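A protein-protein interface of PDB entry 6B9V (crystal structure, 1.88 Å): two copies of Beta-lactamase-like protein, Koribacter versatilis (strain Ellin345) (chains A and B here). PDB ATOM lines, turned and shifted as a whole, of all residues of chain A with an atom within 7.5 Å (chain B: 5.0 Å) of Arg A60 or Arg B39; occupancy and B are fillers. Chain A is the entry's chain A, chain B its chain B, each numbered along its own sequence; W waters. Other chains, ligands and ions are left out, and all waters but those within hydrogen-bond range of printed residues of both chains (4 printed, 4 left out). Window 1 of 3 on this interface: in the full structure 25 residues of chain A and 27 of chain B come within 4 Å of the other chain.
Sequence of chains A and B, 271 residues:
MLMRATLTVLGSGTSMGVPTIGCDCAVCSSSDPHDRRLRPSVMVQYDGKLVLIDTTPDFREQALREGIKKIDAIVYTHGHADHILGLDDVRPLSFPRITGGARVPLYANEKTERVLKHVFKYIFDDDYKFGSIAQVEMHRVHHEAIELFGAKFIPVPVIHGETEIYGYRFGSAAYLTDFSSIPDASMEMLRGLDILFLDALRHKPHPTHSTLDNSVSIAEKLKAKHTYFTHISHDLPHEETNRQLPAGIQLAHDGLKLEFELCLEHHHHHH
The guanidinium group of Arg A60 sits at hydrogen-bond distance from the backbone carbonyl oxygen of Pro B19, 2.8 Å away.
The side-chain carboxylate (OD1) of Asp A89 is in salt-bridge range of the guanidinium group (NH1) of Arg B39, at 2.7 Å.
SD of Met B16 sits close to OD1 of Asp A89 (3.6 Å).
NE of Arg A60 lies within hydrogen-bond range of O of Met B16.
NH2 of Arg A60 lies close to O of Val B18 (3.3 Å).
N of Arg B37 lies within hydrogen-bond range of O of Val B18 (2.8 Å).
The guanidinium group (NE) of Arg B37 lies within hydrogen-bond range of the side-chain hydroxyl (OG) of Ser B12, 2.7 Å away.
N of Gly B13 lies within hydrogen-bond range of O of Leu B38 (2.9 Å).
NE of Arg B39 is in salt-bridge range of OD2 of Asp B58 (2.7 Å).
The backbone carbonyl oxygen (O) of Arg B39 is in hydrogen-bond range of the side-chain amide nitrogen (NE2) of Gln B62.
The guanidinium group (NH1) of Arg B39 is in hydrogen-bond range of the backbone carbonyl oxygen (O) of Ser B15 (3.2 Å).
Phe A59 touches Ile B21 (CE2 to CD1, 3.9 Å).
Arg A60 touches Gly B17 (NH2 to C, 3.8 Å).
Arg A60 touches Ile B21.
Arg A60 touches Arg B37.
Arg B39 touches Arg A60.
CG2 of Ile B21 touches CD2 of Leu A64 (3.7 Å).
Asp A88 touches Met B16 (O to CE, 3.7 Å).
Asp A89 touches Ile B21.
Met B16 touches Pro A92 (SD to CG, 3.6 Å).
Pro A92 touches Ile B21.
Arg A60 touches eight residues of chain B.
Of the printed residues of chain B, Leu A64 touches Ile B21 (3.7 Å).
Of the printed residues of chain B, Pro A92 touches Met B16 (3.6 Å) and Ile B21 (3.97 Å).
Printed residues of chain A within 4 Å of Gly B17: Arg A60.
Of the printed residues of chain A, Val B18 touches Arg A60.
Of the printed residues of chain A, Ile B21 touches Phe A59, Arg A60, Leu A64, Asp A89 and Pro A92.
Of chain A, only Arg A60 and Asp A89 come within 4 Å of Arg B39.
The nearest residue of chain B that does not touch Arg A60 is Asp B58 (4.7 Å).
The nearest residue of chain A that does not touch Arg B39 is Asp A88 (4.9 Å).
The nearest printed residue of chain A that does not touch Met B16 is Val A90 (5.9 Å).
Hydrophobic or aromatic side chains of chain B that line the printed part of chain A: Met B16, Pro B19, Ile B21 and Leu B38.
Of the 18 printed residues of chain A, 6 touch a printed residue of chain B.
Hydrophobic or aromatic side chains of chain A that line the printed part of chain B: Phe A59, Leu A64 and Pro A92.
Positions printed for both chains: 38, 56, 57, 58 and 62.
Of the 16 pairs that touch across the chains among the printed residues, none has its exchanged pair printed and touching as well.
Water W4 lies within hydrogen-bond range of the backbone carbonyl oxygen of Ile B21 (2.7 Å) and the backbone carbonyl oxygen of Pro A92 (3.3 Å).
Water W2 lies within hydrogen-bond range of the side-chain carboxylate of Asp B58 (2.7 Å) and the guanidinium group of Arg A60 (2.9 Å).
Water W3 lies within hydrogen-bond range of the side-chain carboxylate of Asp A88, the backbone carbonyl oxygen of Ser B15 and the backbone NH of Asp B82.
Water W1 bridges the backbone carbonyl oxygen (O) of Asp A89 and the side-chain sulfur (SD) of Met B16.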
ATOM      1  N   LEU A  38      14.823  39.333 -23.189  1.00  0.00           N
ATOM      2  CA  LEU A  38      15.840  38.750 -22.304  1.00  0.00           C
ATOM      3  C   LEU A  38      17.234  39.276 -22.660  1.00  0.00           C
ATOM      4  O   LEU A  38      17.400  40.008 -23.647  1.00  0.00           O
ATOM      5  CB  LEU A  38      15.819  37.222 -22.391  1.00  0.00           C
ATOM      6  CG  LEU A  38      14.453  36.598 -22.108  1.00  0.00           C
ATOM      7  CD1 LEU A  38      14.513  35.064 -22.193  1.00  0.00           C
ATOM      8  CD2 LEU A  38      13.947  37.044 -20.727  1.00  0.00           C
ATOM      9  N   THR A  56      24.025  34.296 -21.279  1.00  0.00           N
ATOM     10  CA  THR A  56      23.422  35.339 -20.457  1.00  0.00           C
ATOM     11  C   THR A  56      22.821  34.738 -19.193  1.00  0.00           C
ATOM     12  O   THR A  56      22.609  33.539 -19.122  1.00  0.00           O
ATOM     13  CB  THR A  56      22.305  36.113 -21.214  1.00  0.00           C
ATOM     14  OG1 THR A  56      21.066  35.377 -21.163  1.00  0.00           O
ATOM     15  CG2 THR A  56      22.709  36.401 -22.668  1.00  0.00           C
ATOM     16  N   PRO A  57      22.560  35.576 -18.188  1.00  0.00           N
ATOM     17  CA  PRO A  57      21.845  35.086 -17.007  1.00  0.00           C
ATOM     18  C   PRO A  57      20.491  34.462 -17.343  1.00  0.00           C
ATOM     19  O   PRO A  57      19.945  33.752 -16.496  1.00  0.00           O
ATOM     20  CB  PRO A  57      21.666  36.347 -16.153  1.00  0.00           C
ATOM     21  CG  PRO A  57      21.958  37.534 -17.118  1.00  0.00           C
ATOM     22  CD  PRO A  57      22.997  36.974 -18.030  1.00  0.00           C
ATOM     23  N   ASP A  58      19.958  34.712 -18.538  1.00  0.00           N
ATOM     24  CA  ASP A  58      18.703  34.069 -18.956  1.00  0.00           C
ATOM     25  C   ASP A  58      18.905  32.778 -19.740  1.00  0.00           C
ATOM     26  O   ASP A  58      17.968  32.275 -20.348  1.00  0.00           O
ATOM     27  CB  ASP A  58      17.858  35.045 -19.798  1.00  0.00           C
ATOM     28  CG  ASP A  58      17.489  36.292 -19.030  1.00  0.00           C
ATOM     29  OD1 ASP A  58      17.089  36.163 -17.850  1.00  0.00           O
ATOM     30  OD2 ASP A  58      17.609  37.411 -19.586  1.00  0.00           O
ATOM     31  N   PHE A  59      20.108  32.219 -19.698  1.00  0.00           N
ATOM     32  CA  PHE A  59      20.391  31.080 -20.566  1.00  0.00           C
ATOM     33  C   PHE A  59      19.465  29.882 -20.331  1.00  0.00           C
ATOM     34  O   PHE A  59      19.011  29.274 -21.289  1.00  0.00           O
ATOM     35  CB  PHE A  59      21.844  30.617 -20.439  1.00  0.00           C
ATOM     36  CG  PHE A  59      22.111  29.355 -21.218  1.00  0.00           C
ATOM     37  CD1 PHE A  59      22.171  29.384 -22.605  1.00  0.00           C
ATOM     38  CD2 PHE A  59      22.224  28.137 -20.570  1.00  0.00           C
ATOM     39  CE1 PHE A  59      22.366  28.223 -23.332  1.00  0.00           C
ATOM     40  CE2 PHE A  59      22.416  26.956 -21.301  1.00  0.00           C
ATOM     41  CZ  PHE A  59      22.492  27.005 -22.675  1.00  0.00           C
ATOM     42  N   ARG A  60      19.173  29.525 -19.083  1.00  0.00           N
ATOM     43  CA  ARG A  60      18.265  28.379 -18.882  1.00  0.00           C
ATOM     44  C   ARG A  60      16.929  28.584 -19.628  1.00  0.00           C
ATOM     45  O   ARG A  60      16.490  27.711 -20.397  1.00  0.00           O
ATOM     46  CB  ARG A  60      17.993  28.131 -17.386  1.00  0.00           C
ATOM     47  CG  ARG A  60      16.944  27.023 -17.159  1.00  0.00           C
ATOM     48  CD  ARG A  60      16.820  26.674 -15.671  1.00  0.00           C
ATOM     49  NE  ARG A  60      15.721  25.733 -15.434  1.00  0.00           N
ATOM     50  CZ  ARG A  60      14.445  26.071 -15.299  1.00  0.00           C
ATOM     51  NH1 ARG A  60      14.074  27.345 -15.358  1.00  0.00           N
ATOM     52  NH2 ARG A  60      13.532  25.119 -15.111  1.00  0.00           N
ATOM     53  N   GLU A  61      16.308  29.749 -19.418  1.00  0.00           N
ATOM     54  CA  GLU A  61      15.040  30.086 -20.071  1.00  0.00           C
ATOM     55  C   GLU A  61      15.182  30.064 -21.600  1.00  0.00           C
ATOM     56  O   GLU A  61      14.307  29.555 -22.308  1.00  0.00           O
ATOM     57  CB  GLU A  61      14.533  31.472 -19.613  1.00  0.00           C
ATOM     58  CG  GLU A  61      13.177  31.903 -20.251  1.00  0.00           C
ATOM     59  CD  GLU A  61      12.585  33.235 -19.694  1.00  0.00           C
ATOM     60  OE1 GLU A  61      13.062  33.794 -18.658  1.00  0.00           O
ATOM     61  OE2 GLU A  61      11.604  33.721 -20.303  1.00  0.00           O
ATOM     62  N   GLN A  62      16.278  30.635 -22.099  1.00  0.00           N
ATOM     63  CA  GLN A  62      16.514  30.710 -23.553  1.00  0.00           C
ATOM     64  C   GLN A  62      16.646  29.309 -24.178  1.00  0.00           C
ATOM     65  O   GLN A  62      16.078  29.015 -25.249  1.00  0.00           O
ATOM     66  CB  GLN A  62      17.758  31.579 -23.852  1.00  0.00           C
ATOM     67  CG  GLN A  62      17.536  33.082 -23.482  1.00  0.00           C
ATOM     68  CD  GLN A  62      18.799  33.952 -23.458  1.00  0.00           C
ATOM     69  OE1 GLN A  62      19.881  33.501 -23.099  1.00  0.00           O
ATOM     70  NE2 GLN A  62      18.640  35.245 -23.806  1.00  0.00           N
ATOM     71  N   ALA A  63      17.378  28.442 -23.486  1.00  0.00           N
ATOM     72  CA  ALA A  63      17.577  27.075 -23.943  1.00  0.00           C
ATOM     73  C   ALA A  63      16.274  26.273 -23.912  1.00  0.00           C
ATOM     74  O   ALA A  63      15.963  25.545 -24.849  1.00  0.00           O
ATOM     75  CB  ALA A  63      18.651  26.377 -23.089  1.00  0.00           C
ATOM     76  N   LEU A  64      15.512  26.402 -22.834  1.00  0.00           N
ATOM     77  CA  LEU A  64      14.254  25.662 -22.721  1.00  0.00           C
ATOM     78  C   LEU A  64      13.284  26.108 -23.794  1.00  0.00           C
ATOM     79  O   LEU A  64      12.637  25.290 -24.440  1.00  0.00           O
ATOM     80  CB  LEU A  64      13.631  25.858 -21.329  1.00  0.00           C
ATOM     81  CG  LEU A  64      14.374  25.191 -20.179  1.00  0.00           C
ATOM     82  CD1 LEU A  64      13.756  25.631 -18.853  1.00  0.00           C
ATOM     83  CD2 LEU A  64      14.310  23.650 -20.339  1.00  0.00           C
ATOM     84  N   ARG A  65      13.212  27.425 -23.978  1.00  0.00           N
ATOM     85  CA  ARG A  65      12.409  28.076 -25.003  1.00  0.00           C
ATOM     86  C   ARG A  65      12.658  27.511 -26.395  1.00  0.00           C
ATOM     87  O   ARG A  65      11.730  27.332 -27.202  1.00  0.00           O
ATOM     88  CB  ARG A  65      12.760  29.572 -25.014  1.00  0.00           C
ATOM     89  CG  ARG A  65      11.682  30.508 -25.332  1.00  0.00           C
ATOM     90  CD  ARG A  65      11.900  31.742 -24.500  1.00  0.00           C
ATOM     91  NE  ARG A  65      12.989  32.596 -24.977  1.00  0.00           N
ATOM     92  CZ  ARG A  65      12.849  33.912 -25.045  1.00  0.00           C
ATOM     93  NH1 ARG A  65      11.691  34.435 -24.675  1.00  0.00           N
ATOM     94  NH2 ARG A  65      13.825  34.695 -25.477  1.00  0.00           N
ATOM     95  N   GLU A  66      13.930  27.284 -26.699  1.00  0.00           N
ATOM     96  CA  GLU A  66      14.275  26.834 -28.041  1.00  0.00           C
ATOM     97  C   GLU A  66      14.550  25.334 -28.160  1.00  0.00           C
ATOM     98  O   GLU A  66      14.948  24.856 -29.231  1.00  0.00           O
ATOM     99  CB  GLU A  66      15.485  27.614 -28.538  1.00  0.00           C
ATOM    100  CG  GLU A  66      15.188  29.086 -28.757  1.00  0.00           C
ATOM    101  CD  GLU A  66      14.363  29.320 -30.009  1.00  0.00           C
ATOM    102  OE1 GLU A  66      13.818  30.435 -30.176  1.00  0.00           O
ATOM    103  OE2 GLU A  66      14.266  28.383 -30.831  1.00  0.00           O
ATOM    104  N   ILE A  68      16.932  23.492 -26.823  1.00  0.00           N
ATOM    105  CA  ILE A  68      18.343  23.124 -26.960  1.00  0.00           C
ATOM    106  C   ILE A  68      18.672  21.865 -26.155  1.00  0.00           C
ATOM    107  O   ILE A  68      18.416  21.800 -24.952  1.00  0.00           O
ATOM    108  CB  ILE A  68      19.272  24.261 -26.511  1.00  0.00           C
ATOM    109  CG1 ILE A  68      19.096  25.483 -27.428  1.00  0.00           C
ATOM    110  CG2 ILE A  68      20.738  23.789 -26.491  1.00  0.00           C
ATOM    111  CD1 ILE A  68      19.872  26.708 -26.960  1.00  0.00           C
ATOM    112  N   GLY A  86      25.171  33.086 -17.192  1.00  0.00           N
ATOM    113  CA  GLY A  86      24.441  31.850 -17.484  1.00  0.00           C
ATOM    114  C   GLY A  86      25.276  30.577 -17.651  1.00  0.00           C
ATOM    115  O   GLY A  86      24.751  29.448 -17.878  1.00  0.00           O
ATOM    116  N   ASP A  88      26.791  28.944 -15.504  1.00  0.00           N
ATOM    117  CA  ASP A  88      26.378  28.005 -14.462  1.00  0.00           C
ATOM    118  C   ASP A  88      25.286  27.072 -14.998  1.00  0.00           C
ATOM    119  O   ASP A  88      25.296  25.852 -14.752  1.00  0.00           O
ATOM    120  CB  ASP A  88      25.882  28.773 -13.222  1.00  0.00           C
ATOM    121  CG  ASP A  88      25.226  27.870 -12.201  1.00  0.00           C
ATOM    122  OD1 ASP A  88      25.947  27.046 -11.606  1.00  0.00           O
ATOM    123  OD2 ASP A  88      23.997  27.991 -11.990  1.00  0.00           O
ATOM    124  N   ASP A  89      24.365  27.638 -15.768  1.00  0.00           N
ATOM    125  CA  ASP A  89      23.217  26.883 -16.260  1.00  0.00           C
ATOM    126  C   ASP A  89      23.542  26.080 -17.502  1.00  0.00           C
ATOM    127  O   ASP A  89      22.719  25.288 -17.950  1.00  0.00           O
ATOM    128  CB  ASP A  89      22.037  27.820 -16.513  1.00  0.00           C
ATOM    129  CG  ASP A  89      21.231  28.061 -15.241  1.00  0.00           C
ATOM    130  OD1 ASP A  89      21.051  27.085 -14.478  1.00  0.00           O
ATOM    131  OD2 ASP A  89      20.793  29.194 -14.994  1.00  0.00           O
ATOM    132  N   VAL A  90      24.739  26.265 -18.052  1.00  0.00           N
ATOM    133  CA  VAL A  90      25.210  25.324 -19.087  1.00  0.00           C
ATOM    134  C   VAL A  90      25.554  23.891 -18.546  1.00  0.00           C
ATOM    135  O   VAL A  90      25.538  22.908 -19.288  1.00  0.00           O
ATOM    136  CB  VAL A  90      26.444  25.919 -19.834  1.00  0.00           C
ATOM    137  CG1 VAL A  90      27.050  24.925 -20.819  1.00  0.00           C
ATOM    138  CG2 VAL A  90      26.041  27.199 -20.564  1.00  0.00           C
ATOM    139  N   PRO A  92      24.203  21.186 -17.051  1.00  0.00           N
ATOM    140  CA  PRO A  92      23.567  19.898 -17.381  1.00  0.00           C
ATOM    141  C   PRO A  92      23.727  19.460 -18.845  1.00  0.00           C
ATOM    142  O   PRO A  92      23.437  18.306 -19.165  1.00  0.00           O
ATOM    143  CB  PRO A  92      22.079  20.143 -17.071  1.00  0.00           C
ATOM    144  CG  PRO A  92      22.043  21.395 -16.249  1.00  0.00           C
ATOM    145  CD  PRO A  92      23.200  22.212 -16.720  1.00  0.00           C
ATOM    146  N   LEU B  10       8.782  31.999  -4.299  1.00  0.00           N
ATOM    147  CA  LEU B  10       9.250  32.541  -5.574  1.00  0.00           C
ATOM    148  C   LEU B  10       9.788  31.427  -6.476  1.00  0.00           C
ATOM    149  O   LEU B  10       9.697  31.503  -7.704  1.00  0.00           O
ATOM    150  CB  LEU B  10      10.328  33.604  -5.339  1.00  0.00           C
ATOM    151  CG  LEU B  10       9.904  34.778  -4.448  1.00  0.00           C
ATOM    152  CD1 LEU B  10      11.067  35.759  -4.196  1.00  0.00           C
ATOM    153  CD2 LEU B  10       8.708  35.509  -5.051  1.00  0.00           C
ATOM    154  N   GLY B  11      10.379  30.408  -5.861  1.00  0.00           N
ATOM    155  CA  GLY B  11      10.808  29.216  -6.579  1.00  0.00           C
ATOM    156  C   GLY B  11      10.822  28.019  -5.637  1.00  0.00           C
ATOM    157  O   GLY B  11      11.226  28.145  -4.477  1.00  0.00           O
ATOM    158  N   SER B  12      10.350  26.877  -6.135  1.00  0.00           N
ATOM    159  CA  SER B  12      10.259  25.635  -5.371  1.00  0.00           C
ATOM    160  C   SER B  12      11.204  24.569  -5.924  1.00  0.00           C
ATOM    161  O   SER B  12      11.157  23.424  -5.491  1.00  0.00           O
ATOM    162  CB  SER B  12       8.830  25.076  -5.394  1.00  0.00           C
ATOM    163  OG  SER B  12       8.437  24.801  -6.737  1.00  0.00           O
ATOM    164  N   GLY B  13      12.045  24.939  -6.883  1.00  0.00           N
ATOM    165  CA  GLY B  13      12.828  23.955  -7.621  1.00  0.00           C
ATOM    166  C   GLY B  13      14.233  23.721  -7.101  1.00  0.00           C
ATOM    167  O   GLY B  13      14.701  24.441  -6.216  1.00  0.00           O
ATOM    168  N   THR B  14      14.901  22.700  -7.639  1.00  0.00           N
ATOM    169  CA  THR B  14      16.273  22.399  -7.261  1.00  0.00           C
ATOM    170  C   THR B  14      17.246  23.322  -8.017  1.00  0.00           C
ATOM    171  O   THR B  14      16.825  24.310  -8.665  1.00  0.00           O
ATOM    172  CB  THR B  14      16.609  20.910  -7.527  1.00  0.00           C
ATOM    173  OG1 THR B  14      17.935  20.618  -7.074  1.00  0.00           O
ATOM    174  CG2 THR B  14      16.470  20.581  -9.013  1.00  0.00           C
ATOM    175  N   SER B  15      18.537  23.019  -7.931  1.00  0.00           N
ATOM    176  CA  SER B  15      19.552  23.990  -8.359  1.00  0.00           C
ATOM    177  C   SER B  15      19.500  24.249  -9.863  1.00  0.00           C
ATOM    178  O   SER B  15      19.794  25.363 -10.318  1.00  0.00           O
ATOM    179  CB  SER B  15      20.948  23.520  -7.955  1.00  0.00           C
ATOM    180  OG  SER B  15      21.317  22.364  -8.684  1.00  0.00           O
ATOM    181  N   MET B  16      19.106  23.240 -10.641  1.00  0.00           N
ATOM    182  CA  MET B  16      18.977  23.454 -12.083  1.00  0.00           C
ATOM    183  C   MET B  16      17.511  23.629 -12.510  1.00  0.00           C
ATOM    184  O   MET B  16      17.194  23.639 -13.697  1.00  0.00           O
ATOM    185  CB  MET B  16      19.646  22.312 -12.847  1.00  0.00           C
ATOM    186  CG  MET B  16      21.183  22.331 -12.733  1.00  0.00           C
ATOM    187  SD  MET B  16      21.958  23.780 -13.527  1.00  0.00           S
ATOM    188  CE  MET B  16      23.078  24.357 -12.252  1.00  0.00           C
ATOM    189  N   GLY B  17      16.620  23.800 -11.537  1.00  0.00           N
ATOM    190  CA  GLY B  17      15.213  23.991 -11.844  1.00  0.00           C
ATOM    191  C   GLY B  17      14.498  22.749 -12.361  1.00  0.00           C
ATOM    192  O   GLY B  17      15.086  21.683 -12.481  1.00  0.00           O
ATOM    193  N   VAL B  18      13.210  22.901 -12.640  1.00  0.00           N
ATOM    194  CA  VAL B  18      12.415  21.902 -13.334  1.00  0.00           C
ATOM    195  C   VAL B  18      11.601  22.651 -14.385  1.00  0.00           C
ATOM    196  O   VAL B  18      10.862  23.576 -14.045  1.00  0.00           O
ATOM    197  CB  VAL B  18      11.480  21.129 -12.376  1.00  0.00           C
ATOM    198  CG1 VAL B  18      10.810  19.958 -13.107  1.00  0.00           C
ATOM    199  CG2 VAL B  18      12.265  20.602 -11.167  1.00  0.00           C
ATOM    200  N   PRO B  19      11.763  22.295 -15.668  1.00  0.00           N
ATOM    201  CA  PRO B  19      12.609  21.222 -16.224  1.00  0.00           C
ATOM    202  C   PRO B  19      14.106  21.459 -16.070  1.00  0.00           C
ATOM    203  O   PRO B  19      14.544  22.581 -15.791  1.00  0.00           O
ATOM    204  CB  PRO B  19      12.258  21.225 -17.723  1.00  0.00           C
ATOM    205  CG  PRO B  19      10.967  22.003 -17.833  1.00  0.00           C
ATOM    206  CD  PRO B  19      10.971  22.979 -16.703  1.00  0.00           C
ATOM    207  N   ILE B  21      17.396  21.505 -18.354  1.00  0.00           N
ATOM    208  CA  ILE B  21      17.640  21.623 -19.782  1.00  0.00           C
ATOM    209  C   ILE B  21      18.210  20.332 -20.346  1.00  0.00           C
ATOM    210  O   ILE B  21      19.027  19.670 -19.711  1.00  0.00           O
ATOM    211  CB  ILE B  21      18.585  22.782 -20.102  1.00  0.00           C
ATOM    212  CG1 ILE B  21      19.916  22.620 -19.375  1.00  0.00           C
ATOM    213  CG2 ILE B  21      17.935  24.104 -19.724  1.00  0.00           C
ATOM    214  CD1 ILE B  21      20.913  23.687 -19.791  1.00  0.00           C
ATOM    215  N   ARG B  37       9.331  24.797 -12.088  1.00  0.00           N
ATOM    216  CA  ARG B  37       9.908  25.245 -10.819  1.00  0.00           C
ATOM    217  C   ARG B  37      11.173  26.059 -11.016  1.00  0.00           C
ATOM    218  O   ARG B  37      12.209  25.526 -11.476  1.00  0.00           O
ATOM    219  CB  ARG B  37      10.242  24.057  -9.914  1.00  0.00           C
ATOM    220  CG  ARG B  37       9.310  22.851 -10.030  1.00  0.00           C
ATOM    221  CD  ARG B  37       9.466  21.863  -8.862  1.00  0.00           C
ATOM    222  NE  ARG B  37       8.605  22.287  -7.774  1.00  0.00           N
ATOM    223  CZ  ARG B  37       7.481  21.679  -7.414  1.00  0.00           C
ATOM    224  NH1 ARG B  37       7.082  20.563  -8.010  1.00  0.00           N
ATOM    225  NH2 ARG B  37       6.777  22.181  -6.426  1.00  0.00           N
ATOM    226  N   LEU B  38      11.096  27.344 -10.669  1.00  0.00           N
ATOM    227  CA  LEU B  38      12.277  28.207 -10.665  1.00  0.00           C
ATOM    228  C   LEU B  38      13.148  27.885  -9.460  1.00  0.00           C
ATOM    229  O   LEU B  38      12.740  27.113  -8.596  1.00  0.00           O
ATOM    230  CB  LEU B  38      11.869  29.691 -10.666  1.00  0.00           C
ATOM    231  CG  LEU B  38      11.149  30.075 -11.971  1.00  0.00           C
ATOM    232  CD1 LEU B  38      10.907  31.570 -12.056  1.00  0.00           C
ATOM    233  CD2 LEU B  38      11.918  29.595 -13.201  1.00  0.00           C
ATOM    234  N   ARG B  39      14.369  28.424  -9.420  1.00  0.00           N
ATOM    235  CA  ARG B  39      15.314  28.113  -8.346  1.00  0.00           C
ATOM    236  C   ARG B  39      14.825  28.584  -6.948  1.00  0.00           C
ATOM    237  O   ARG B  39      13.964  29.411  -6.877  1.00  0.00           O
ATOM    238  CB  ARG B  39      16.720  28.596  -8.672  1.00  0.00           C
ATOM    239  CG  ARG B  39      17.564  27.580  -9.424  1.00  0.00           C
ATOM    240  CD  ARG B  39      17.024  27.209 -10.802  1.00  0.00           C
ATOM    241  NE  ARG B  39      17.153  28.227 -11.817  1.00  0.00           N
ATOM    242  CZ  ARG B  39      18.168  28.332 -12.647  1.00  0.00           C
ATOM    243  NH1 ARG B  39      19.164  27.489 -12.586  1.00  0.00           N
ATOM    244  NH2 ARG B  39      18.225  29.290 -13.503  1.00  0.00           N
ATOM    245  N   PRO B  40      15.320  28.009  -5.854  1.00  0.00           N
ATOM    246  CA  PRO B  40      14.594  28.115  -4.571  1.00  0.00           C
ATOM    247  C   PRO B  40      14.760  29.423  -3.802  1.00  0.00           C
ATOM    248  O   PRO B  40      15.875  29.801  -3.422  1.00  0.00           O
ATOM    249  CB  PRO B  40      15.173  26.963  -3.750  1.00  0.00           C
ATOM    250  CG  PRO B  40      16.567  26.771  -4.297  1.00  0.00           C
ATOM    251  CD  PRO B  40      16.453  27.066  -5.775  1.00  0.00           C
ATOM    252  N   SER B  41      13.633  30.075  -3.536  1.00  0.00           N
ATOM    253  CA  SER B  41      13.629  31.334  -2.788  1.00  0.00           C
ATOM    254  C   SER B  41      12.227  31.629  -2.281  1.00  0.00           C
ATOM    255  O   SER B  41      11.231  31.261  -2.913  1.00  0.00           O
ATOM    256  CB  SER B  41      14.130  32.479  -3.676  1.00  0.00           C
ATOM    257  OG  SER B  41      14.095  33.739  -3.015  1.00  0.00           O
ATOM    258  N   THR B  56      18.137  34.024  -6.213  1.00  0.00           N
ATOM    259  CA  THR B  56      18.448  32.973  -7.172  1.00  0.00           C
ATOM    260  C   THR B  56      18.742  33.544  -8.547  1.00  0.00           C
ATOM    261  O   THR B  56      18.355  34.669  -8.836  1.00  0.00           O
ATOM    262  CB  THR B  56      17.286  31.974  -7.334  1.00  0.00           C
ATOM    263  OG1 THR B  56      16.249  32.585  -8.121  1.00  0.00           O
ATOM    264  CG2 THR B  56      16.750  31.519  -5.986  1.00  0.00           C
ATOM    265  N   PRO B  57      19.378  32.752  -9.424  1.00  0.00           N
ATOM    266  CA  PRO B  57      19.562  33.257 -10.798  1.00  0.00           C
ATOM    267  C   PRO B  57      18.251  33.638 -11.504  1.00  0.00           C
ATOM    268  O   PRO B  57      18.296  34.377 -12.487  1.00  0.00           O
ATOM    269  CB  PRO B  57      20.248  32.089 -11.523  1.00  0.00           C
ATOM    270  CG  PRO B  57      20.057  30.862 -10.592  1.00  0.00           C
ATOM    271  CD  PRO B  57      20.032  31.447  -9.215  1.00  0.00           C
ATOM    272  N   ASP B  58      17.111  33.174 -11.000  1.00  0.00           N
ATOM    273  CA  ASP B  58      15.825  33.547 -11.580  1.00  0.00           C
ATOM    274  C   ASP B  58      15.215  34.791 -10.926  1.00  0.00           C
ATOM    275  O   ASP B  58      14.042  35.091 -11.152  1.00  0.00           O
ATOM    276  CB  ASP B  58      14.835  32.364 -11.482  1.00  0.00           C
ATOM    277  CG  ASP B  58      15.322  31.134 -12.222  1.00  0.00           C
ATOM    278  OD1 ASP B  58      15.838  31.260 -13.360  1.00  0.00           O
ATOM    279  OD2 ASP B  58      15.187  30.019 -11.676  1.00  0.00           O
ATOM    280  N   GLN B  62      11.348  36.171 -11.097  1.00  0.00           N
ATOM    281  CA  GLN B  62      10.583  36.054  -9.839  1.00  0.00           C
ATOM    282  C   GLN B  62       9.991  37.413  -9.393  1.00  0.00           C
ATOM    283  O   GLN B  62       8.782  37.528  -9.083  1.00  0.00           O
ATOM    284  CB  GLN B  62      11.472  35.434  -8.739  1.00  0.00           C
ATOM    285  CG  GLN B  62      11.750  33.916  -8.983  1.00  0.00           C
ATOM    286  CD  GLN B  62      12.900  33.309  -8.155  1.00  0.00           C
ATOM    287  OE1 GLN B  62      13.867  33.984  -7.789  1.00  0.00           O
ATOM    288  NE2 GLN B  62      12.795  32.003  -7.878  1.00  0.00           N
ATOM    289  N   ASP B  82      22.933  28.598  -7.052  1.00  0.00           N
ATOM    290  CA  ASP B  82      21.483  28.665  -7.229  1.00  0.00           C
ATOM    291  C   ASP B  82      20.829  29.560  -6.167  1.00  0.00           C
ATOM    292  O   ASP B  82      19.643  29.842  -6.251  1.00  0.00           O
ATOM    293  CB  ASP B  82      20.845  27.253  -7.230  1.00  0.00           C
ATOM    294  CG  ASP B  82      21.264  26.404  -6.043  1.00  0.00           C
ATOM    295  OD1 ASP B  82      20.389  25.714  -5.469  1.00  0.00           O
ATOM    296  OD2 ASP B  82      22.462  26.393  -5.698  1.00  0.00           O
HETATM  297  O   HOH W   1      20.599  24.813 -16.317  1.00  0.00           O
HETATM  298  O   HOH W   2      15.292  29.935 -15.643  1.00  0.00           O
HETATM  299  O   HOH W   3      22.658  26.762  -9.979  1.00  0.00           O
HETATM  300  O   HOH W   4      20.256  17.355 -19.123  1.00  0.00           O
